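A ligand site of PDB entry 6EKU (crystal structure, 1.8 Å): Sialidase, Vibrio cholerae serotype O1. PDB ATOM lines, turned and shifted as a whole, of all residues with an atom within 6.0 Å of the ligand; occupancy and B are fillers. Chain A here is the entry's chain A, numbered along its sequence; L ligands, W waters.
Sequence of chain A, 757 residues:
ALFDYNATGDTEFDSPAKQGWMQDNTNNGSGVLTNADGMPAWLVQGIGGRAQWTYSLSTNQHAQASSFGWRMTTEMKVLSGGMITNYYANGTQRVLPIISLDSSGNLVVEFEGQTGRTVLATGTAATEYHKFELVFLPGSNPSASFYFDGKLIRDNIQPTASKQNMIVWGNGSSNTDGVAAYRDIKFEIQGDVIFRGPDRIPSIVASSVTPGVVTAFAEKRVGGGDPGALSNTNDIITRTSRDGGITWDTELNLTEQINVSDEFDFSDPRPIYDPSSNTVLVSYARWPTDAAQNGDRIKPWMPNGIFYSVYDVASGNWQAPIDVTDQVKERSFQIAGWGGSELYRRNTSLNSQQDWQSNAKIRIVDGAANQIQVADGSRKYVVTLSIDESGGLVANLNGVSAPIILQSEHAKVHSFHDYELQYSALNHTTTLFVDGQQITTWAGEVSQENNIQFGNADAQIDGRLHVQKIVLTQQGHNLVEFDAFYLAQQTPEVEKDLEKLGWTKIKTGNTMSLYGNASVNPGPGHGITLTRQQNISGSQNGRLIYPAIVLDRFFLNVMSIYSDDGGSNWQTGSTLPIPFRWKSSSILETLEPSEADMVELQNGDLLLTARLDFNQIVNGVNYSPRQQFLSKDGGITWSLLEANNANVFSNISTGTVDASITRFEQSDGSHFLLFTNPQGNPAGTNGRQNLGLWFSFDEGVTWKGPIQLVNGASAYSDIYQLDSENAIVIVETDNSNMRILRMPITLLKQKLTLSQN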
ATOM      1  N   ARG A 200     -37.583  -1.932 -25.359  1.00  0.00           N
ATOM      2  CA  ARG A 200     -36.609  -2.128 -24.279  1.00  0.00           C
ATOM      3  C   ARG A 200     -36.729  -1.115 -23.141  1.00  0.00           C
ATOM      4  O   ARG A 200     -37.505  -0.155 -23.222  1.00  0.00           O
ATOM      5  CB  ARG A 200     -35.165  -2.063 -24.825  1.00  0.00           C
ATOM      6  CG  ARG A 200     -34.660  -3.293 -25.589  1.00  0.00           C
ATOM      7  CD  ARG A 200     -33.134  -3.309 -25.611  1.00  0.00           C
ATOM      8  NE  ARG A 200     -32.569  -3.471 -24.267  1.00  0.00           N
ATOM      9  CZ  ARG A 200     -31.347  -3.081 -23.898  1.00  0.00           C
ATOM     10  NH1 ARG A 200     -30.549  -2.473 -24.773  1.00  0.00           N
ATOM     11  NH2 ARG A 200     -30.937  -3.283 -22.648  1.00  0.00           N
ATOM     12  N   ILE A 201     -35.940  -1.364 -22.089  1.00  0.00           N
ATOM     13  CA  ILE A 201     -35.650  -0.406 -20.997  1.00  0.00           C
ATOM     14  C   ILE A 201     -36.852  -0.222 -20.046  1.00  0.00           C
ATOM     15  O   ILE A 201     -37.472   0.835 -19.993  1.00  0.00           O
ATOM     16  CB  ILE A 201     -35.196   0.981 -21.542  1.00  0.00           C
ATOM     17  CG1 ILE A 201     -34.305   0.823 -22.784  1.00  0.00           C
ATOM     18  CG2 ILE A 201     -34.436   1.763 -20.441  1.00  0.00           C
ATOM     19  CD1 ILE A 201     -33.007   0.095 -22.566  1.00  0.00           C
ATOM     20  N   GLU A 219     -39.465   1.644 -23.727  1.00  0.00           N
ATOM     21  CA  GLU A 219     -39.313   2.417 -24.959  1.00  0.00           C
ATOM     22  C   GLU A 219     -39.892   1.619 -26.108  1.00  0.00           C
ATOM     23  O   GLU A 219     -39.457   0.494 -26.354  1.00  0.00           O
ATOM     24  CB  GLU A 219     -37.834   2.719 -25.252  1.00  0.00           C
ATOM     25  CG  GLU A 219     -37.124   3.491 -24.155  1.00  0.00           C
ATOM     26  CD  GLU A 219     -35.643   3.639 -24.425  1.00  0.00           C
ATOM     27  OE1 GLU A 219     -35.195   3.284 -25.549  1.00  0.00           O
ATOM     28  OE2 GLU A 219     -34.912   4.100 -23.521  1.00  0.00           O
ATOM     29  N   ARG A 221     -39.581   0.916 -29.674  1.00  0.00           N
ATOM     30  CA  ARG A 221     -38.497   1.155 -30.603  1.00  0.00           C
ATOM     31  C   ARG A 221     -38.829   0.683 -32.017  1.00  0.00           C
ATOM     32  O   ARG A 221     -38.693  -0.501 -32.328  1.00  0.00           O
ATOM     33  CB  ARG A 221     -37.232   0.477 -30.117  1.00  0.00           C
ATOM     34  CG  ARG A 221     -36.796   0.878 -28.745  1.00  0.00           C
ATOM     35  CD  ARG A 221     -35.666  -0.005 -28.368  1.00  0.00           C
ATOM     36  NE  ARG A 221     -34.754   0.630 -27.459  1.00  0.00           N
ATOM     37  CZ  ARG A 221     -33.465   0.323 -27.409  1.00  0.00           C
ATOM     38  NH1 ARG A 221     -32.983  -0.596 -28.246  1.00  0.00           N
ATOM     39  NH2 ARG A 221     -32.668   0.919 -26.536  1.00  0.00           N
ATOM     40  N   GLY A 225     -33.762   0.035 -32.345  1.00  0.00           N
ATOM     41  CA  GLY A 225     -32.470   0.575 -31.939  1.00  0.00           C
ATOM     42  C   GLY A 225     -32.494   1.577 -30.800  1.00  0.00           C
ATOM     43  O   GLY A 225     -33.560   2.035 -30.379  1.00  0.00           O
ATOM     44  N   ASP A 226     -31.308   1.899 -30.277  1.00  0.00           N
ATOM     45  CA  ASP A 226     -31.152   2.970 -29.296  1.00  0.00           C
ATOM     46  C   ASP A 226     -31.579   4.320 -29.905  1.00  0.00           C
ATOM     47  O   ASP A 226     -31.582   4.482 -31.121  1.00  0.00           O
ATOM     48  CB  ASP A 226     -29.699   3.049 -28.793  1.00  0.00           C
ATOM     49  CG  ASP A 226     -29.418   2.048 -27.680  1.00  0.00           C
ATOM     50  OD1 ASP A 226     -30.377   1.528 -27.079  1.00  0.00           O
ATOM     51  OD2 ASP A 226     -28.222   1.781 -27.397  1.00  0.00           O
ATOM     52  N   PRO A 227     -31.958   5.287 -29.048  1.00  0.00           N
ATOM     53  CA  PRO A 227     -32.294   6.607 -29.576  1.00  0.00           C
ATOM     54  C   PRO A 227     -31.141   7.214 -30.383  1.00  0.00           C
ATOM     55  O   PRO A 227     -29.979   6.937 -30.088  1.00  0.00           O
ATOM     56  CB  PRO A 227     -32.569   7.432 -28.303  1.00  0.00           C
ATOM     57  CG  PRO A 227     -31.843   6.721 -27.233  1.00  0.00           C
ATOM     58  CD  PRO A 227     -31.989   5.268 -27.575  1.00  0.00           C
ATOM     59  N   ASN A 234     -38.364   6.307 -31.793  1.00  0.00           N
ATOM     60  CA  ASN A 234     -38.683   5.667 -30.510  1.00  0.00           C
ATOM     61  C   ASN A 234     -39.588   6.554 -29.664  1.00  0.00           C
ATOM     62  O   ASN A 234     -39.405   7.779 -29.608  1.00  0.00           O
ATOM     63  CB  ASN A 234     -37.424   5.330 -29.707  1.00  0.00           C
ATOM     64  CG  ASN A 234     -36.452   4.455 -30.454  1.00  0.00           C
ATOM     65  OD1 ASN A 234     -36.764   3.890 -31.496  1.00  0.00           O
ATOM     66  ND2 ASN A 234     -35.252   4.296 -29.890  1.00  0.00           N
ATOM     67  N   SER A 267     -36.557   8.353 -24.641  1.00  0.00           N
ATOM     68  CA  SER A 267     -35.903   7.221 -23.966  1.00  0.00           C
ATOM     69  C   SER A 267     -35.999   7.291 -22.453  1.00  0.00           C
ATOM     70  O   SER A 267     -36.379   8.310 -21.888  1.00  0.00           O
ATOM     71  CB  SER A 267     -34.427   7.164 -24.357  1.00  0.00           C
ATOM     72  OG  SER A 267     -33.674   8.119 -23.613  1.00  0.00           O
ATOM     73  N   ASP A 268     -35.633   6.168 -21.822  1.00  0.00           N
ATOM     74  CA  ASP A 268     -35.354   6.136 -20.375  1.00  0.00           C
ATOM     75  C   ASP A 268     -36.503   6.631 -19.500  1.00  0.00           C
ATOM     76  O   ASP A 268     -36.360   7.655 -18.799  1.00  0.00           O
ATOM     77  CB  ASP A 268     -34.080   6.937 -20.071  1.00  0.00           C
ATOM     78  CG  ASP A 268     -32.825   6.315 -20.686  1.00  0.00           C
ATOM     79  OD1 ASP A 268     -32.548   6.543 -21.875  1.00  0.00           O
ATOM     80  OD2 ASP A 268     -32.102   5.581 -19.965  1.00  0.00           O
ATOM     81  N   TRP A 287     -34.661  13.211 -27.514  1.00  0.00           N
ATOM     82  CA  TRP A 287     -33.490  13.336 -28.378  1.00  0.00           C
ATOM     83  C   TRP A 287     -33.931  13.733 -29.761  1.00  0.00           C
ATOM     84  O   TRP A 287     -34.995  13.323 -30.206  1.00  0.00           O
ATOM     85  CB  TRP A 287     -32.718  12.015 -28.470  1.00  0.00           C
ATOM     86  CG  TRP A 287     -32.434  11.379 -27.151  1.00  0.00           C
ATOM     87  CD1 TRP A 287     -33.166  10.400 -26.539  1.00  0.00           C
ATOM     88  CD2 TRP A 287     -31.326  11.662 -26.285  1.00  0.00           C
ATOM     89  NE1 TRP A 287     -32.580  10.061 -25.343  1.00  0.00           N
ATOM     90  CE2 TRP A 287     -31.460  10.816 -25.156  1.00  0.00           C
ATOM     91  CE3 TRP A 287     -30.253  12.547 -26.346  1.00  0.00           C
ATOM     92  CZ2 TRP A 287     -30.543  10.835 -24.100  1.00  0.00           C
ATOM     93  CZ3 TRP A 287     -29.340  12.557 -25.293  1.00  0.00           C
ATOM     94  CH2 TRP A 287     -29.490  11.712 -24.181  1.00  0.00           C
ATOM     95  N   ALA A 292     -27.965  11.261 -30.222  1.00  0.00           N
ATOM     96  CA  ALA A 292     -28.280  11.032 -28.824  1.00  0.00           C
ATOM     97  C   ALA A 292     -27.022  10.812 -27.992  1.00  0.00           C
ATOM     98  O   ALA A 292     -25.929  11.267 -28.359  1.00  0.00           O
ATOM     99  CB  ALA A 292     -29.256   9.822 -28.685  1.00  0.00           C
ATOM    100  N   GLN A 293     -27.180  10.119 -26.882  1.00  0.00           N
ATOM    101  CA  GLN A 293     -26.135  10.043 -25.869  1.00  0.00           C
ATOM    102  C   GLN A 293     -24.954   9.204 -26.341  1.00  0.00           C
ATOM    103  O   GLN A 293     -23.800   9.595 -26.163  1.00  0.00           O
ATOM    104  CB  GLN A 293     -26.725   9.469 -24.571  1.00  0.00           C
ATOM    105  CG  GLN A 293     -25.899   9.689 -23.337  1.00  0.00           C
ATOM    106  CD  GLN A 293     -26.576   9.056 -22.139  1.00  0.00           C
ATOM    107  OE1 GLN A 293     -27.465   9.658 -21.540  1.00  0.00           O
ATOM    108  NE2 GLN A 293     -26.187   7.812 -21.830  1.00  0.00           N
ATOM    109  N   ASN A 294     -25.251   8.062 -26.959  1.00  0.00           N
ATOM    110  CA  ASN A 294     -24.199   7.179 -27.466  1.00  0.00           C
ATOM    111  C   ASN A 294     -23.306   7.878 -28.476  1.00  0.00           C
ATOM    112  O   ASN A 294     -23.779   8.605 -29.359  1.00  0.00           O
ATOM    113  CB  ASN A 294     -24.811   5.926 -28.098  1.00  0.00           C
ATOM    114  CG  ASN A 294     -25.414   5.006 -27.062  1.00  0.00           C
ATOM    115  OD1 ASN A 294     -25.182   5.161 -25.865  1.00  0.00           O
ATOM    116  ND2 ASN A 294     -26.192   4.025 -27.522  1.00  0.00           N
ATOM    117  N   ASN A 521     -30.687  13.188 -19.042  1.00  0.00           N
ATOM    118  CA  ASN A 521     -31.394  11.937 -19.326  1.00  0.00           C
ATOM    119  C   ASN A 521     -31.793  11.310 -17.992  1.00  0.00           C
ATOM    120  O   ASN A 521     -30.927  11.079 -17.151  1.00  0.00           O
ATOM    121  CB  ASN A 521     -30.484  11.020 -20.151  1.00  0.00           C
ATOM    122  CG  ASN A 521     -31.063   9.611 -20.361  1.00  0.00           C
ATOM    123  OD1 ASN A 521     -32.211   9.346 -20.017  1.00  0.00           O
ATOM    124  ND2 ASN A 521     -30.288   8.725 -20.970  1.00  0.00           N
ATOM    125  N   PRO A 524     -32.713   4.769 -16.617  1.00  0.00           N
ATOM    126  CA  PRO A 524     -33.632   3.620 -16.554  1.00  0.00           C
ATOM    127  C   PRO A 524     -33.908   3.128 -15.132  1.00  0.00           C
ATOM    128  O   PRO A 524     -32.985   2.881 -14.380  1.00  0.00           O
ATOM    129  CB  PRO A 524     -32.882   2.554 -17.347  1.00  0.00           C
ATOM    130  CG  PRO A 524     -31.451   2.818 -17.046  1.00  0.00           C
ATOM    131  CD  PRO A 524     -31.323   4.336 -16.883  1.00  0.00           C
ATOM    132  N   LEU A 556     -19.882  11.217 -19.077  1.00  0.00           N
ATOM    133  CA  LEU A 556     -21.114  11.004 -18.338  1.00  0.00           C
ATOM    134  C   LEU A 556     -20.881  11.093 -16.833  1.00  0.00           C
ATOM    135  O   LEU A 556     -19.815  10.751 -16.329  1.00  0.00           O
ATOM    136  CB  LEU A 556     -21.711   9.612 -18.668  1.00  0.00           C
ATOM    137  CG  LEU A 556     -22.073   9.358 -20.131  1.00  0.00           C
ATOM    138  CD1 LEU A 556     -22.450   7.869 -20.306  1.00  0.00           C
ATOM    139  CD2 LEU A 556     -23.219  10.239 -20.560  1.00  0.00           C
ATOM    140  N   SER A 594     -23.382   6.151 -14.930  1.00  0.00           N
ATOM    141  CA  SER A 594     -24.481   6.423 -15.858  1.00  0.00           C
ATOM    142  C   SER A 594     -25.834   5.966 -15.318  1.00  0.00           C
ATOM    143  O   SER A 594     -26.511   6.714 -14.611  1.00  0.00           O
ATOM    144  CB  SER A 594     -24.191   5.760 -17.218  1.00  0.00           C
ATOM    145  OG  SER A 594     -23.967   4.359 -17.103  1.00  0.00           O
ATOM    146  N   GLU A 595     -26.229   4.750 -15.645  1.00  0.00           N
ATOM    147  CA  GLU A 595     -27.541   4.276 -15.246  1.00  0.00           C
ATOM    148  C   GLU A 595     -27.588   3.999 -13.750  1.00  0.00           C
ATOM    149  O   GLU A 595     -26.881   3.133 -13.241  1.00  0.00           O
ATOM    150  CB  GLU A 595     -27.900   3.025 -16.039  1.00  0.00           C
ATOM    151  CG  GLU A 595     -27.939   3.307 -17.529  1.00  0.00           C
ATOM    152  CD  GLU A 595     -28.218   2.082 -18.349  1.00  0.00           C
ATOM    153  OE1 GLU A 595     -27.935   0.964 -17.851  1.00  0.00           O
ATOM    154  OE2 GLU A 595     -28.726   2.235 -19.492  1.00  0.00           O
ATOM    155  N   ARG A 611     -24.261   2.152 -12.491  1.00  0.00           N
ATOM    156  CA  ARG A 611     -23.463   1.510 -13.526  1.00  0.00           C
ATOM    157  C   ARG A 611     -22.255   2.378 -13.860  1.00  0.00           C
ATOM    158  O   ARG A 611     -22.396   3.591 -14.009  1.00  0.00           O
ATOM    159  CB  ARG A 611     -24.334   1.289 -14.763  1.00  0.00           C
ATOM    160  CG  ARG A 611     -23.606   0.835 -16.011  1.00  0.00           C
ATOM    161  CD  ARG A 611     -24.635   0.657 -17.122  1.00  0.00           C
ATOM    162  NE  ARG A 611     -24.039   0.318 -18.405  1.00  0.00           N
ATOM    163  CZ  ARG A 611     -24.724  -0.190 -19.428  1.00  0.00           C
ATOM    164  NH1 ARG A 611     -26.025  -0.437 -19.319  1.00  0.00           N
ATOM    165  NH2 ARG A 611     -24.101  -0.451 -20.573  1.00  0.00           N
ATOM    166  N   ASP A 613     -19.657   3.104 -16.682  1.00  0.00           N
ATOM    167  CA  ASP A 613     -19.457   2.805 -18.108  1.00  0.00           C
ATOM    168  C   ASP A 613     -18.033   3.131 -18.575  1.00  0.00           C
ATOM    169  O   ASP A 613     -17.338   3.954 -17.961  1.00  0.00           O
ATOM    170  CB  ASP A 613     -20.485   3.565 -18.949  1.00  0.00           C
ATOM    171  CG  ASP A 613     -21.787   2.789 -19.122  1.00  0.00           C
ATOM    172  OD1 ASP A 613     -21.745   1.549 -19.265  1.00  0.00           O
ATOM    173  OD2 ASP A 613     -22.861   3.436 -19.117  1.00  0.00           O
ATOM    174  N   PHE A 614     -17.611   2.470 -19.647  1.00  0.00           N
ATOM    175  CA  PHE A 614     -16.295   2.675 -20.243  1.00  0.00           C
ATOM    176  C   PHE A 614     -15.203   2.413 -19.204  1.00  0.00           C
ATOM    177  O   PHE A 614     -15.255   1.403 -18.517  1.00  0.00           O
ATOM    178  CB  PHE A 614     -16.195   4.102 -20.831  1.00  0.00           C
ATOM    179  CG  PHE A 614     -17.429   4.492 -21.621  1.00  0.00           C
ATOM    180  CD1 PHE A 614     -17.714   3.866 -22.828  1.00  0.00           C
ATOM    181  CD2 PHE A 614     -18.317   5.439 -21.132  1.00  0.00           C
ATOM    182  CE1 PHE A 614     -18.860   4.197 -23.545  1.00  0.00           C
ATOM    183  CE2 PHE A 614     -19.445   5.781 -21.839  1.00  0.00           C
ATOM    184  CZ  PHE A 614     -19.730   5.155 -23.045  1.00  0.00           C
ATOM    185  N   THR A 656     -21.379  -4.650 -17.580  1.00  0.00           N
ATOM    186  CA  THR A 656     -22.170  -3.455 -17.313  1.00  0.00           C
ATOM    187  C   THR A 656     -23.607  -3.628 -17.786  1.00  0.00           C
ATOM    188  O   THR A 656     -23.849  -4.105 -18.896  1.00  0.00           O
ATOM    189  CB  THR A 656     -21.575  -2.203 -17.991  1.00  0.00           C
ATOM    190  OG1 THR A 656     -21.217  -2.525 -19.345  1.00  0.00           O
ATOM    191  CG2 THR A 656     -20.328  -1.727 -17.246  1.00  0.00           C
ATOM    192  N   VAL A 657     -24.542  -3.226 -16.936  1.00  0.00           N
ATOM    193  CA  VAL A 657     -25.964  -3.415 -17.192  1.00  0.00           C
ATOM    194  C   VAL A 657     -26.735  -2.578 -16.172  1.00  0.00           C
ATOM    195  O   VAL A 657     -26.196  -2.270 -15.116  1.00  0.00           O
ATOM    196  CB  VAL A 657     -26.358  -4.913 -17.079  1.00  0.00           C
ATOM    197  CG1 VAL A 657     -26.275  -5.363 -15.630  1.00  0.00           C
ATOM    198  CG2 VAL A 657     -27.752  -5.160 -17.648  1.00  0.00           C
ATOM    199  N   ARG A 688     -25.595 -11.149 -19.650  1.00  0.00           N
ATOM    200  CA  ARG A 688     -26.961 -10.768 -19.310  1.00  0.00           C
ATOM    201  C   ARG A 688     -27.834 -12.032 -19.239  1.00  0.00           C
ATOM    202  O   ARG A 688     -28.676 -12.291 -20.109  1.00  0.00           O
ATOM    203  CB  ARG A 688     -27.477  -9.722 -20.304  1.00  0.00           C
ATOM    204  CG  ARG A 688     -26.776  -8.386 -20.075  1.00  0.00           C
ATOM    205  CD  ARG A 688     -27.067  -7.336 -21.139  1.00  0.00           C
ATOM    206  NE  ARG A 688     -26.289  -6.128 -20.859  1.00  0.00           N
ATOM    207  CZ  ARG A 688     -26.567  -4.926 -21.340  1.00  0.00           C
ATOM    208  NH1 ARG A 688     -27.620  -4.756 -22.128  1.00  0.00           N
ATOM    209  NH2 ARG A 688     -25.802  -3.889 -21.030  1.00  0.00           N
ATOM    210  N   TYR A 716     -31.880  -5.678 -18.467  1.00  0.00           N
ATOM    211  CA  TYR A 716     -32.394  -4.604 -17.604  1.00  0.00           C
ATOM    212  C   TYR A 716     -33.596  -5.108 -16.797  1.00  0.00           C
ATOM    213  O   TYR A 716     -34.389  -5.904 -17.289  1.00  0.00           O
ATOM    214  CB  TYR A 716     -32.812  -3.369 -18.403  1.00  0.00           C
ATOM    215  CG  TYR A 716     -31.683  -2.532 -18.959  1.00  0.00           C
ATOM    216  CD1 TYR A 716     -30.450  -3.093 -19.283  1.00  0.00           C
ATOM    217  CD2 TYR A 716     -31.853  -1.158 -19.155  1.00  0.00           C
ATOM    218  CE1 TYR A 716     -29.424  -2.320 -19.800  1.00  0.00           C
ATOM    219  CE2 TYR A 716     -30.821  -0.364 -19.677  1.00  0.00           C
ATOM    220  CZ  TYR A 716     -29.613  -0.954 -19.974  1.00  0.00           C
ATOM    221  OH  TYR A 716     -28.584  -0.202 -20.456  1.00  0.00           O
ATOM    222  N   GLU A 732     -36.087  -7.623 -18.776  1.00  0.00           N
ATOM    223  CA  GLU A 732     -35.835  -7.973 -20.186  1.00  0.00           C
ATOM    224  C   GLU A 732     -35.296  -9.393 -20.260  1.00  0.00           C
ATOM    225  O   GLU A 732     -34.342  -9.723 -19.552  1.00  0.00           O
ATOM    226  CB  GLU A 732     -34.828  -7.032 -20.836  1.00  0.00           C
ATOM    227  CG  GLU A 732     -35.167  -5.544 -20.816  1.00  0.00           C
ATOM    228  CD  GLU A 732     -34.066  -4.705 -21.462  1.00  0.00           C
ATOM    229  OE1 GLU A 732     -32.888  -5.091 -21.345  1.00  0.00           O
ATOM    230  OE2 GLU A 732     -34.376  -3.664 -22.098  1.00  0.00           O
HETATM  231  C1  LIG L   1     -27.298  -1.255 -22.961  1.00  0.00           C
HETATM  232  O1  LIG L   1     -26.167  -1.455 -22.464  1.00  0.00           O
HETATM  233  O2  LIG L   1     -28.168  -2.135 -23.158  1.00  0.00           O
HETATM  234  C2  LIG L   1     -27.618   0.182 -23.442  1.00  0.00           C
HETATM  235  C3  LIG L   1     -29.107   0.494 -23.274  1.00  0.00           C
HETATM  236  C4  LIG L   1     -29.444   1.995 -23.261  1.00  0.00           C
HETATM  237  C5  LIG L   1     -28.235   2.860 -23.586  1.00  0.00           C
HETATM  238  N1  LIG L   1     -28.632   4.252 -23.300  1.00  0.00           N
HETATM  239  C6  LIG L   1     -28.827   5.173 -24.252  1.00  0.00           C
HETATM  240  O3  LIG L   1     -28.683   4.955 -25.449  1.00  0.00           O
HETATM  241  C7  LIG L   1     -29.247   6.565 -23.748  1.00  0.00           C
HETATM  242  C8  LIG L   1     -27.072   2.471 -22.666  1.00  0.00           C
HETATM  243  O4  LIG L   1     -26.736   1.061 -22.724  1.00  0.00           O
HETATM  244  C9  LIG L   1     -25.784   3.236 -23.007  1.00  0.00           C
HETATM  245  O5  LIG L   1     -25.383   2.941 -24.327  1.00  0.00           O
HETATM  246  C10 LIG L   1     -24.667   2.752 -22.078  1.00  0.00           C
HETATM  247  O6  LIG L   1     -25.014   3.010 -20.715  1.00  0.00           O
HETATM  248  C11 LIG L   1     -23.313   3.410 -22.433  1.00  0.00           C
HETATM  249  O7  LIG L   1     -23.270   4.754 -21.919  1.00  0.00           O
HETATM  250  N2  LIG L   1     -30.537   2.269 -24.210  1.00  0.00           N
HETATM  251  C12 LIG L   1     -31.572   3.085 -23.963  1.00  0.00           C
HETATM  252  N3  LIG L   1     -31.694   3.694 -22.789  1.00  0.00           N
HETATM  253  N4  LIG L   1     -32.507   3.272 -24.904  1.00  0.00           N
HETATM  254  O   HOH W   1     -24.043   6.679 -23.718  1.00  0.00           O
HETATM  255  O   HOH W   2     -28.036   6.991 -27.082  1.00  0.00           O
HETATM  256  O   HOH W   3     -26.840   5.354 -20.262  1.00  0.00           O
HETATM  257  O   HOH W   4     -29.746   4.510 -20.566  1.00  0.00           O
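O6 of the ligand lies within hydrogen-bond range of OD2 of Asp 613, 2.7 Å away.
N4 of the ligand lies within salt-bridge range of OE1 of Glu 219, at 2.8 Å.
The side-chain carboxylate (OD1) of Asp 226 is in salt-bridge range of a nitrogen (N2) of the ligand (3.0 Å).
OH of Tyr 716 sits close to O4 of the ligand.
NH2 of Arg 611 is in salt-bridge range of O1 of the ligand, at 3.0 Å.
The side-chain carboxylate (OD1) of Asp 268 is in salt-bridge range of a nitrogen (N3) of the ligand (3.1 Å).
NH2 of Arg 688 is in salt-bridge range of O1 of the ligand (2.8 Å).
The side-chain amide oxygen (OD1) of Asn 294 is in hydrogen-bond range of an oxygen (O5) of the ligand, 2.7 Å away.
NH1 of Arg 200 lies within salt-bridge range of O2 of the ligand (2.9 Å).
OD1 of Asp 268 sits at hydrogen-bond distance from ND2 of Asn 521, at 3.3 Å.
The backbone carbonyl oxygen (O) of Gly 225 lies close to the guanidinium group (NH1) of Arg 221 (3.4 Å).
N of Glu 219 lies within hydrogen-bond range of O of Arg 200 (2.7 Å).
ND2 of Asn 294 is in hydrogen-bond range of OD2 of Asp 226, at 3.0 Å.
The guanidinium group of Arg 221 lies within salt-bridge range of the side-chain carboxylate of Glu 219 (3.3 Å).
ND2 of Asn 521 lies within hydrogen-bond range of OE1 of Gln 293 (3.0 Å).
The side-chain carboxylate of Asp 613 is in hydrogen-bond range of the side-chain hydroxyl of Ser 594, at 2.5 Å.
The guanidinium group (NH2) of Arg 221 is in salt-bridge range of the side-chain carboxylate (OD1) of Asp 226 (2.4 Å).
The guanidinium group (NH2) of Arg 221 sits close to a nitrogen (N4) of the ligand (2.9 Å).
Residues that only touch the ligand: Pro 227, Glu 595, Ile 201, Leu 556, Asn 521, Phe 614, Gln 293 and Ser 594.
Hydrophobic or aromatic side chains within 4 Å of the ligand: Ile 201, Pro 227, Leu 556, Phe 614 and Tyr 716.
Within 4 Å of the ligand: Arg 200, Ile 201, Glu 219, Arg 221, Asp 226, Pro 227, Asp 268, Gln 293, Asn 294, Asn 521, Leu 556, Ser 594, Glu 595, Arg 611, Asp 613, Phe 614, Arg 688 and Tyr 716.
The nearest printed residue that does not touch the ligand is Ser 267 (4.4 Å).
Water W2 lies within hydrogen-bond range of an oxygen (O3) of the ligand, the backbone NH (N) of Asn 294 and the backbone NH (N) of Gln 293.
Water W1 lies within hydrogen-bond range of an oxygen (O7) of the ligand (2.7 Å), the side-chain amide oxygen of Asn 294 (2.9 Å) and the side-chain amide nitrogen of Gln 293 (3.1 Å).
Water W4 lies within hydrogen-bond range of the side-chain carboxylate (OD2) of Asp 268 (2.7 Å), the side-chain carboxylate (OE2) of Glu 595 (2.7 Å) and a nitrogen (N1) of the ligand (3.0 Å).
Water W3 bridges the side-chain amide nitrogen (NE2) of Gln 293 (3.0 Å) and an oxygen (O6) of the ligand (3.0 Å).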
